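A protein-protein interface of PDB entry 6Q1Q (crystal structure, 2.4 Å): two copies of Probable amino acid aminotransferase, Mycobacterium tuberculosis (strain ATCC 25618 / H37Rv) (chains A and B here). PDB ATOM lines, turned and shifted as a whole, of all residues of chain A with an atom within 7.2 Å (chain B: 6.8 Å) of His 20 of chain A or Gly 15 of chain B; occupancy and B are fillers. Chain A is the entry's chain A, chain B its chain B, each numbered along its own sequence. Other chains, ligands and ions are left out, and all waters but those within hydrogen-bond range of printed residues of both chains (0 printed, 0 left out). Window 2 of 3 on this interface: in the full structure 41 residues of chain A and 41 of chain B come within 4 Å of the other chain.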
ATOM      1  N   PRO A  17     -29.716  17.499   0.203  1.00  0.00           N
ATOM      2  CA  PRO A  17     -28.564  17.395   1.105  1.00  0.00           C
ATOM      3  C   PRO A  17     -28.725  16.267   2.110  1.00  0.00           C
ATOM      4  O   PRO A  17     -29.832  15.928   2.530  1.00  0.00           O
ATOM      5  CB  PRO A  17     -28.543  18.756   1.808  1.00  0.00           C
ATOM      6  CG  PRO A  17     -29.972  19.211   1.758  1.00  0.00           C
ATOM      7  CD  PRO A  17     -30.490  18.730   0.430  1.00  0.00           C
ATOM      8  N   LEU A  18     -27.592  15.682   2.492  1.00  0.00           N
ATOM      9  CA  LEU A  18     -27.544  14.555   3.415  1.00  0.00           C
ATOM     10  C   LEU A  18     -27.013  14.923   4.791  1.00  0.00           C
ATOM     11  O   LEU A  18     -27.557  14.470   5.798  1.00  0.00           O
ATOM     12  CB  LEU A  18     -26.675  13.432   2.837  1.00  0.00           C
ATOM     13  CG  LEU A  18     -26.511  12.201   3.733  1.00  0.00           C
ATOM     14  CD1 LEU A  18     -27.867  11.602   4.070  1.00  0.00           C
ATOM     15  CD2 LEU A  18     -25.601  11.170   3.085  1.00  0.00           C
ATOM     16  N   LEU A  19     -25.970  15.747   4.857  1.00  0.00           N
ATOM     17  CA  LEU A  19     -25.216  15.962   6.082  1.00  0.00           C
ATOM     18  C   LEU A  19     -25.575  17.293   6.727  1.00  0.00           C
ATOM     19  O   LEU A  19     -25.781  18.297   6.037  1.00  0.00           O
ATOM     20  CB  LEU A  19     -23.716  15.917   5.792  1.00  0.00           C
ATOM     21  CG  LEU A  19     -23.290  14.684   4.997  1.00  0.00           C
ATOM     22  CD1 LEU A  19     -21.849  14.803   4.553  1.00  0.00           C
ATOM     23  CD2 LEU A  19     -23.501  13.421   5.819  1.00  0.00           C
ATOM     24  N   HIS A  20     -25.649  17.289   8.055  1.00  0.00           N
ATOM     25  CA  HIS A  20     -25.874  18.512   8.809  1.00  0.00           C
ATOM     26  C   HIS A  20     -24.609  19.368   8.828  1.00  0.00           C
ATOM     27  O   HIS A  20     -23.493  18.890   8.599  1.00  0.00           O
ATOM     28  CB  HIS A  20     -26.320  18.188  10.236  1.00  0.00           C
ATOM     29  CG  HIS A  20     -27.703  17.622  10.320  1.00  0.00           C
ATOM     30  ND1 HIS A  20     -27.953  16.266  10.350  1.00  0.00           N
ATOM     31  CD2 HIS A  20     -28.912  18.228  10.375  1.00  0.00           C
ATOM     32  CE1 HIS A  20     -29.255  16.062  10.423  1.00  0.00           C
ATOM     33  NE2 HIS A  20     -29.861  17.235  10.438  1.00  0.00           N
ATOM     34  N   ALA A  21     -24.798  20.658   9.112  1.00  0.00           N
ATOM     35  CA  ALA A  21     -23.694  21.609   9.053  1.00  0.00           C
ATOM     36  C   ALA A  21     -22.646  21.381  10.140  1.00  0.00           C
ATOM     37  O   ALA A  21     -21.530  21.896  10.013  1.00  0.00           O
ATOM     38  CB  ALA A  21     -24.226  23.039   9.141  1.00  0.00           C
ATOM     39  N   ASP A  22     -22.967  20.630  11.196  1.00  0.00           N
ATOM     40  CA  ASP A  22     -22.034  20.397  12.294  1.00  0.00           C
ATOM     41  C   ASP A  22     -21.468  18.978  12.304  1.00  0.00           C
ATOM     42  O   ASP A  22     -21.025  18.499  13.353  1.00  0.00           O
ATOM     43  CB  ASP A  22     -22.700  20.711  13.636  1.00  0.00           C
ATOM     44  CG  ASP A  22     -23.943  19.874  13.884  1.00  0.00           C
ATOM     45  OD1 ASP A  22     -24.382  19.166  12.955  1.00  0.00           O
ATOM     46  OD2 ASP A  22     -24.479  19.919  15.014  1.00  0.00           O
ATOM     47  N   ASP A  23     -21.470  18.295  11.162  1.00  0.00           N
ATOM     48  CA  ASP A  23     -20.905  16.954  11.087  1.00  0.00           C
ATOM     49  C   ASP A  23     -19.380  17.018  11.098  1.00  0.00           C
ATOM     50  O   ASP A  23     -18.777  17.775  10.332  1.00  0.00           O
ATOM     51  CB  ASP A  23     -21.402  16.246   9.827  1.00  0.00           C
ATOM     52  CG  ASP A  23     -21.209  14.744   9.884  1.00  0.00           C
ATOM     53  OD1 ASP A  23     -20.044  14.290   9.857  1.00  0.00           O
ATOM     54  OD2 ASP A  23     -22.225  14.019   9.959  1.00  0.00           O
ATOM     55  N   LEU A  24     -18.753  16.209  11.961  1.00  0.00           N
ATOM     56  CA  LEU A  24     -17.295  16.221  12.074  1.00  0.00           C
ATOM     57  C   LEU A  24     -16.589  15.840  10.779  1.00  0.00           C
ATOM     58  O   LEU A  24     -15.377  16.055  10.675  1.00  0.00           O
ATOM     59  CB  LEU A  24     -16.814  15.294  13.198  1.00  0.00           C
ATOM     60  CG  LEU A  24     -16.956  15.715  14.668  1.00  0.00           C
ATOM     61  CD1 LEU A  24     -16.656  17.196  14.833  1.00  0.00           C
ATOM     62  CD2 LEU A  24     -18.303  15.364  15.277  1.00  0.00           C
ATOM     63  N   ALA A  26     -17.296  17.278   7.820  1.00  0.00           N
ATOM     64  CA  ALA A  26     -17.099  18.534   7.107  1.00  0.00           C
ATOM     65  C   ALA A  26     -16.331  19.563   7.924  1.00  0.00           C
ATOM     66  O   ALA A  26     -15.478  20.272   7.378  1.00  0.00           O
ATOM     67  CB  ALA A  26     -18.449  19.122   6.697  1.00  0.00           C
ATOM     68  N   VAL A  27     -16.604  19.648   9.227  1.00  0.00           N
ATOM     69  CA  VAL A  27     -15.978  20.687  10.037  1.00  0.00           C
ATOM     70  C   VAL A  27     -14.549  20.317  10.419  1.00  0.00           C
ATOM     71  O   VAL A  27     -13.724  21.204  10.665  1.00  0.00           O
ATOM     72  CB  VAL A  27     -16.835  20.991  11.280  1.00  0.00           C
ATOM     73  CG1 VAL A  27     -18.228  21.439  10.863  1.00  0.00           C
ATOM     74  CG2 VAL A  27     -16.918  19.781  12.191  1.00  0.00           C
ATOM     75  N   ARG A  99     -21.984  13.917  14.400  1.00  0.00           N
ATOM     76  CA  ARG A  99     -22.187  15.334  14.647  1.00  0.00           C
ATOM     77  C   ARG A  99     -21.568  15.738  15.983  1.00  0.00           C
ATOM     78  O   ARG A  99     -21.351  14.909  16.868  1.00  0.00           O
ATOM     79  CB  ARG A  99     -23.676  15.680  14.630  1.00  0.00           C
ATOM     80  CG  ARG A  99     -24.469  14.988  13.530  1.00  0.00           C
ATOM     81  CD  ARG A  99     -25.897  15.514  13.499  1.00  0.00           C
ATOM     82  NE  ARG A  99     -25.953  16.955  13.744  1.00  0.00           N
ATOM     83  CZ  ARG A  99     -26.983  17.577  14.311  1.00  0.00           C
ATOM     84  NH1 ARG A  99     -28.048  16.885  14.695  1.00  0.00           N
ATOM     85  NH2 ARG A  99     -26.948  18.890  14.498  1.00  0.00           N
ATOM     86  N   THR A 106     -21.696   9.000  11.419  1.00  0.00           N
ATOM     87  CA  THR A 106     -22.311   9.152  10.110  1.00  0.00           C
ATOM     88  C   THR A 106     -21.717   8.118   9.165  1.00  0.00           C
ATOM     89  O   THR A 106     -20.494   7.966   9.092  1.00  0.00           O
ATOM     90  CB  THR A 106     -22.089  10.565   9.566  1.00  0.00           C
ATOM     91  OG1 THR A 106     -22.787  11.507  10.387  1.00  0.00           O
ATOM     92  CG2 THR A 106     -22.589  10.676   8.133  1.00  0.00           C
ATOM     93  N   ASN B   1     -29.274  22.392  17.445  1.00  0.00           N
ATOM     94  CA  ASN B   1     -28.112  22.565  18.309  1.00  0.00           C
ATOM     95  C   ASN B   1     -27.425  23.905  18.063  1.00  0.00           C
ATOM     96  O   ASN B   1     -26.936  24.546  18.994  1.00  0.00           O
ATOM     97  CB  ASN B   1     -27.110  21.426  18.093  1.00  0.00           C
ATOM     98  CG  ASN B   1     -25.913  21.515  19.025  1.00  0.00           C
ATOM     99  OD1 ASN B   1     -25.048  22.378  18.870  1.00  0.00           O
ATOM    100  ND2 ASN B   1     -25.854  20.608  19.993  1.00  0.00           N
ATOM    101  N   LEU B  12     -30.762  29.123   8.265  1.00  0.00           N
ATOM    102  CA  LEU B  12     -31.191  27.773   7.950  1.00  0.00           C
ATOM    103  C   LEU B  12     -32.301  27.336   8.887  1.00  0.00           C
ATOM    104  O   LEU B  12     -32.438  27.844  10.002  1.00  0.00           O
ATOM    105  CB  LEU B  12     -30.022  26.797   8.090  1.00  0.00           C
ATOM    106  CG  LEU B  12     -30.146  25.426   7.412  1.00  0.00           C
ATOM    107  CD1 LEU B  12     -30.104  25.499   5.892  1.00  0.00           C
ATOM    108  CD2 LEU B  12     -29.114  24.442   7.969  1.00  0.00           C
ATOM    109  N   GLN B  13     -33.127  26.424   8.401  1.00  0.00           N
ATOM    110  CA  GLN B  13     -34.034  25.741   9.299  1.00  0.00           C
ATOM    111  C   GLN B  13     -33.194  25.085  10.391  1.00  0.00           C
ATOM    112  O   GLN B  13     -32.070  24.646  10.124  1.00  0.00           O
ATOM    113  CB  GLN B  13     -34.848  24.697   8.529  1.00  0.00           C
ATOM    114  CG  GLN B  13     -35.740  25.271   7.416  1.00  0.00           C
ATOM    115  CD  GLN B  13     -34.975  25.901   6.255  1.00  0.00           C
ATOM    116  OE1 GLN B  13     -33.956  25.380   5.794  1.00  0.00           O
ATOM    117  NE2 GLN B  13     -35.463  27.052   5.796  1.00  0.00           N
ATOM    118  N   PRO B  14     -33.704  24.985  11.617  1.00  0.00           N
ATOM    119  CA  PRO B  14     -32.876  24.418  12.700  1.00  0.00           C
ATOM    120  C   PRO B  14     -32.464  22.968  12.488  1.00  0.00           C
ATOM    121  O   PRO B  14     -31.276  22.641  12.622  1.00  0.00           O
ATOM    122  CB  PRO B  14     -33.775  24.598  13.930  1.00  0.00           C
ATOM    123  CG  PRO B  14     -34.595  25.817  13.597  1.00  0.00           C
ATOM    124  CD  PRO B  14     -34.890  25.690  12.132  1.00  0.00           C
ATOM    125  N   GLY B  15     -33.400  22.090  12.146  1.00  0.00           N
ATOM    126  CA  GLY B  15     -33.063  20.687  11.989  1.00  0.00           C
ATOM    127  C   GLY B  15     -32.808  20.192  10.579  1.00  0.00           C
ATOM    128  O   GLY B  15     -32.853  18.982  10.333  1.00  0.00           O
ATOM    129  N   MET B  16     -32.537  21.099   9.642  1.00  0.00           N
ATOM    130  CA  MET B  16     -32.467  20.511   8.310  1.00  0.00           C
ATOM    131  C   MET B  16     -31.018  20.333   7.865  1.00  0.00           C
ATOM    132  O   MET B  16     -30.174  21.189   8.147  1.00  0.00           O
ATOM    133  CB  MET B  16     -33.200  21.383   7.288  1.00  0.00           C
ATOM    134  CG  MET B  16     -34.731  21.325   7.337  1.00  0.00           C
ATOM    135  SD  MET B  16     -35.478  19.683   7.430  1.00  0.00           S
ATOM    136  CE  MET B  16     -35.851  19.563   9.184  1.00  0.00           C
ATOM    137  N   PRO B  17     -30.696  19.234   7.180  1.00  0.00           N
ATOM    138  CA  PRO B  17     -29.318  19.037   6.713  1.00  0.00           C
ATOM    139  C   PRO B  17     -28.943  20.054   5.645  1.00  0.00           C
ATOM    140  O   PRO B  17     -29.781  20.505   4.860  1.00  0.00           O
ATOM    141  CB  PRO B  17     -29.336  17.610   6.151  1.00  0.00           C
ATOM    142  CG  PRO B  17     -30.762  17.382   5.773  1.00  0.00           C
ATOM    143  CD  PRO B  17     -31.567  18.106   6.814  1.00  0.00           C
ATOM    144  N   LEU B  18     -27.661  20.414   5.624  1.00  0.00           N
ATOM    145  CA  LEU B  18     -27.151  21.473   4.757  1.00  0.00           C
ATOM    146  C   LEU B  18     -26.309  20.987   3.588  1.00  0.00           C
ATOM    147  O   LEU B  18     -26.425  21.531   2.488  1.00  0.00           O
ATOM    148  CB  LEU B  18     -26.322  22.463   5.581  1.00  0.00           C
ATOM    149  CG  LEU B  18     -25.687  23.616   4.803  1.00  0.00           C
ATOM    150  CD1 LEU B  18     -26.751  24.421   4.070  1.00  0.00           C
ATOM    151  CD2 LEU B  18     -24.872  24.504   5.727  1.00  0.00           C
ATOM    152  N   LEU B  19     -25.439  20.005   3.791  1.00  0.00           N
ATOM    153  CA  LEU B  19     -24.428  19.657   2.803  1.00  0.00           C
ATOM    154  C   LEU B  19     -24.800  18.386   2.051  1.00  0.00           C
ATOM    155  O   LEU B  19     -25.337  17.439   2.634  1.00  0.00           O
ATOM    156  CB  LEU B  19     -23.061  19.489   3.469  1.00  0.00           C
ATOM    157  CG  LEU B  19     -22.639  20.662   4.356  1.00  0.00           C
ATOM    158  CD1 LEU B  19     -21.386  20.329   5.139  1.00  0.00           C
ATOM    159  CD2 LEU B  19     -22.429  21.915   3.517  1.00  0.00           C
ATOM    160  N   TYR B 108     -20.696  28.963   4.605  1.00  0.00           N
ATOM    161  CA  TYR B 108     -21.723  29.306   5.578  1.00  0.00           C
ATOM    162  C   TYR B 108     -21.057  29.693   6.890  1.00  0.00           C
ATOM    163  O   TYR B 108     -19.857  29.490   7.091  1.00  0.00           O
ATOM    164  CB  TYR B 108     -22.715  28.155   5.785  1.00  0.00           C
ATOM    165  CG  TYR B 108     -22.100  26.851   6.255  1.00  0.00           C
ATOM    166  CD1 TYR B 108     -21.596  25.929   5.345  1.00  0.00           C
ATOM    167  CD2 TYR B 108     -22.037  26.538   7.607  1.00  0.00           C
ATOM    168  CE1 TYR B 108     -21.041  24.734   5.768  1.00  0.00           C
ATOM    169  CE2 TYR B 108     -21.485  25.344   8.040  1.00  0.00           C
ATOM    170  CZ  TYR B 108     -20.987  24.447   7.116  1.00  0.00           C
ATOM    171  OH  TYR B 108     -20.435  23.258   7.543  1.00  0.00           O
ATOM    172  N   MET B 110     -21.488  29.467  11.175  1.00  0.00           N
ATOM    173  CA  MET B 110     -22.065  28.623  12.207  1.00  0.00           C
ATOM    174  C   MET B 110     -21.692  29.183  13.566  1.00  0.00           C
ATOM    175  O   MET B 110     -20.519  29.479  13.815  1.00  0.00           O
ATOM    176  CB  MET B 110     -21.573  27.180  12.084  1.00  0.00           C
ATOM    177  CG  MET B 110     -22.385  26.185  12.892  1.00  0.00           C
ATOM    178  SD  MET B 110     -22.221  24.490  12.300  1.00  0.00           S
ATOM    179  CE  MET B 110     -20.459  24.402  11.997  1.00  0.00           C
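The backbone NH of Leu 18 of chain A lies within hydrogen-bond range of the backbone carbonyl oxygen of Leu 19 of chain B. The backbone NH of Leu 19 of chain B sits at hydrogen-bond distance from the backbone carbonyl oxygen of Leu 19 of chain A (2.8 Å). The backbone carbonyl oxygen (O) of Ala 21 of chain A lies within hydrogen-bond range of the side-chain hydroxyl (OH) of Tyr 108 of chain B (3.0 Å). The side-chain sulfur of Met 110 of chain B lies close to the backbone carbonyl oxygen of Ala 21 of chain A (3.5 Å). A ring nitrogen (NE2) of His 20 of chain A lies within hydrogen-bond range of the backbone carbonyl oxygen of Gly 15 of chain B, at 3.5 Å. N of Leu 18 of chain B sits at hydrogen-bond distance from O of Leu 19 of chain A.
Among the printed residues, pairs that only touch across the chains: Pro 17 of chain A with Pro 17 of chain B, Pro 17 of chain A with Leu 18 of chain B, Pro 17 of chain A with Leu 19 of chain B, Leu 18 of chain A with Pro 17 of chain B, Leu 19 of chain A with Pro 17 of chain B, His 20 of chain A with Met 16 of chain B, His 20 of chain A with Pro 17 of chain B, Ala 21 of chain A with Leu 18 of chain B, Ala 26 of chain A with Leu 19 of chain B and Val 27 of chain A with Met 110 of chain B.
Of chain B, only Gly 15 (3.5 Å), Met 16 (3.9 Å) and Pro 17 (3.8 Å) come within 4 Å of His 20 of chain A. Printed residues of chain A within 4 Å of Met 16 of chain B: His 20. Of the printed residues of chain B, Ala 26 of chain A touches Leu 19 (3.5 Å). Asn 1 of chain B touches none of the printed residues of chain A. Asp 22 of chain A touches none of the printed residues of chain B. The nearest residue of chain B that does not touch His 20 of chain A is Leu 18 of chain B (4.1 Å). The nearest residue of chain A that does not touch Gly 15 of chain B is Arg 99 of chain A (6.8 Å). The nearest printed residue of chain B that does not touch Pro 17 of chain A is Met 16 of chain B (6.3 Å).
Printed residues of chain B that touch a printed residue of chain A: Gly 15, Met 16, Pro 17, Leu 18, Leu 19, Tyr 108 and Met 110. Hydrophobic or aromatic side chains of chain B that line the printed part of chain A: Pro 17, Leu 18, Leu 19, Tyr 108 and Met 110. Of the 12 printed residues of chain A, 7 touch a printed residue of chain B. Hydrophobic or aromatic side chains of chain A that line the printed part of chain B: Pro 17, Leu 19, His 20, Ala 21, Ala 26 and Val 27. Among the printed residues, 16 pairs touch across the chains. Among the printed residues, no Asp or Glu carboxylate lies within 4 Å of a Lys or Arg side-chain nitrogen of the other chain.
Pro 17 of chain B touches its own counterpart, Pro 17 of chain A. Pro 17 of chain A touches Leu 19 of chain B, and with the chains exchanged Leu 19 of chain A touches Pro 17 of chain B. Leu 18 of chain A touches Leu 19 of chain B, and with the chains exchanged Leu 19 of chain A touches Leu 18 of chain B. Leu 19 of chain A touches its own counterpart, Leu 19 of chain B. Of the 16 pairs that touch across the chains among the printed residues, 8 have their exchanged pair printed and touching as well.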
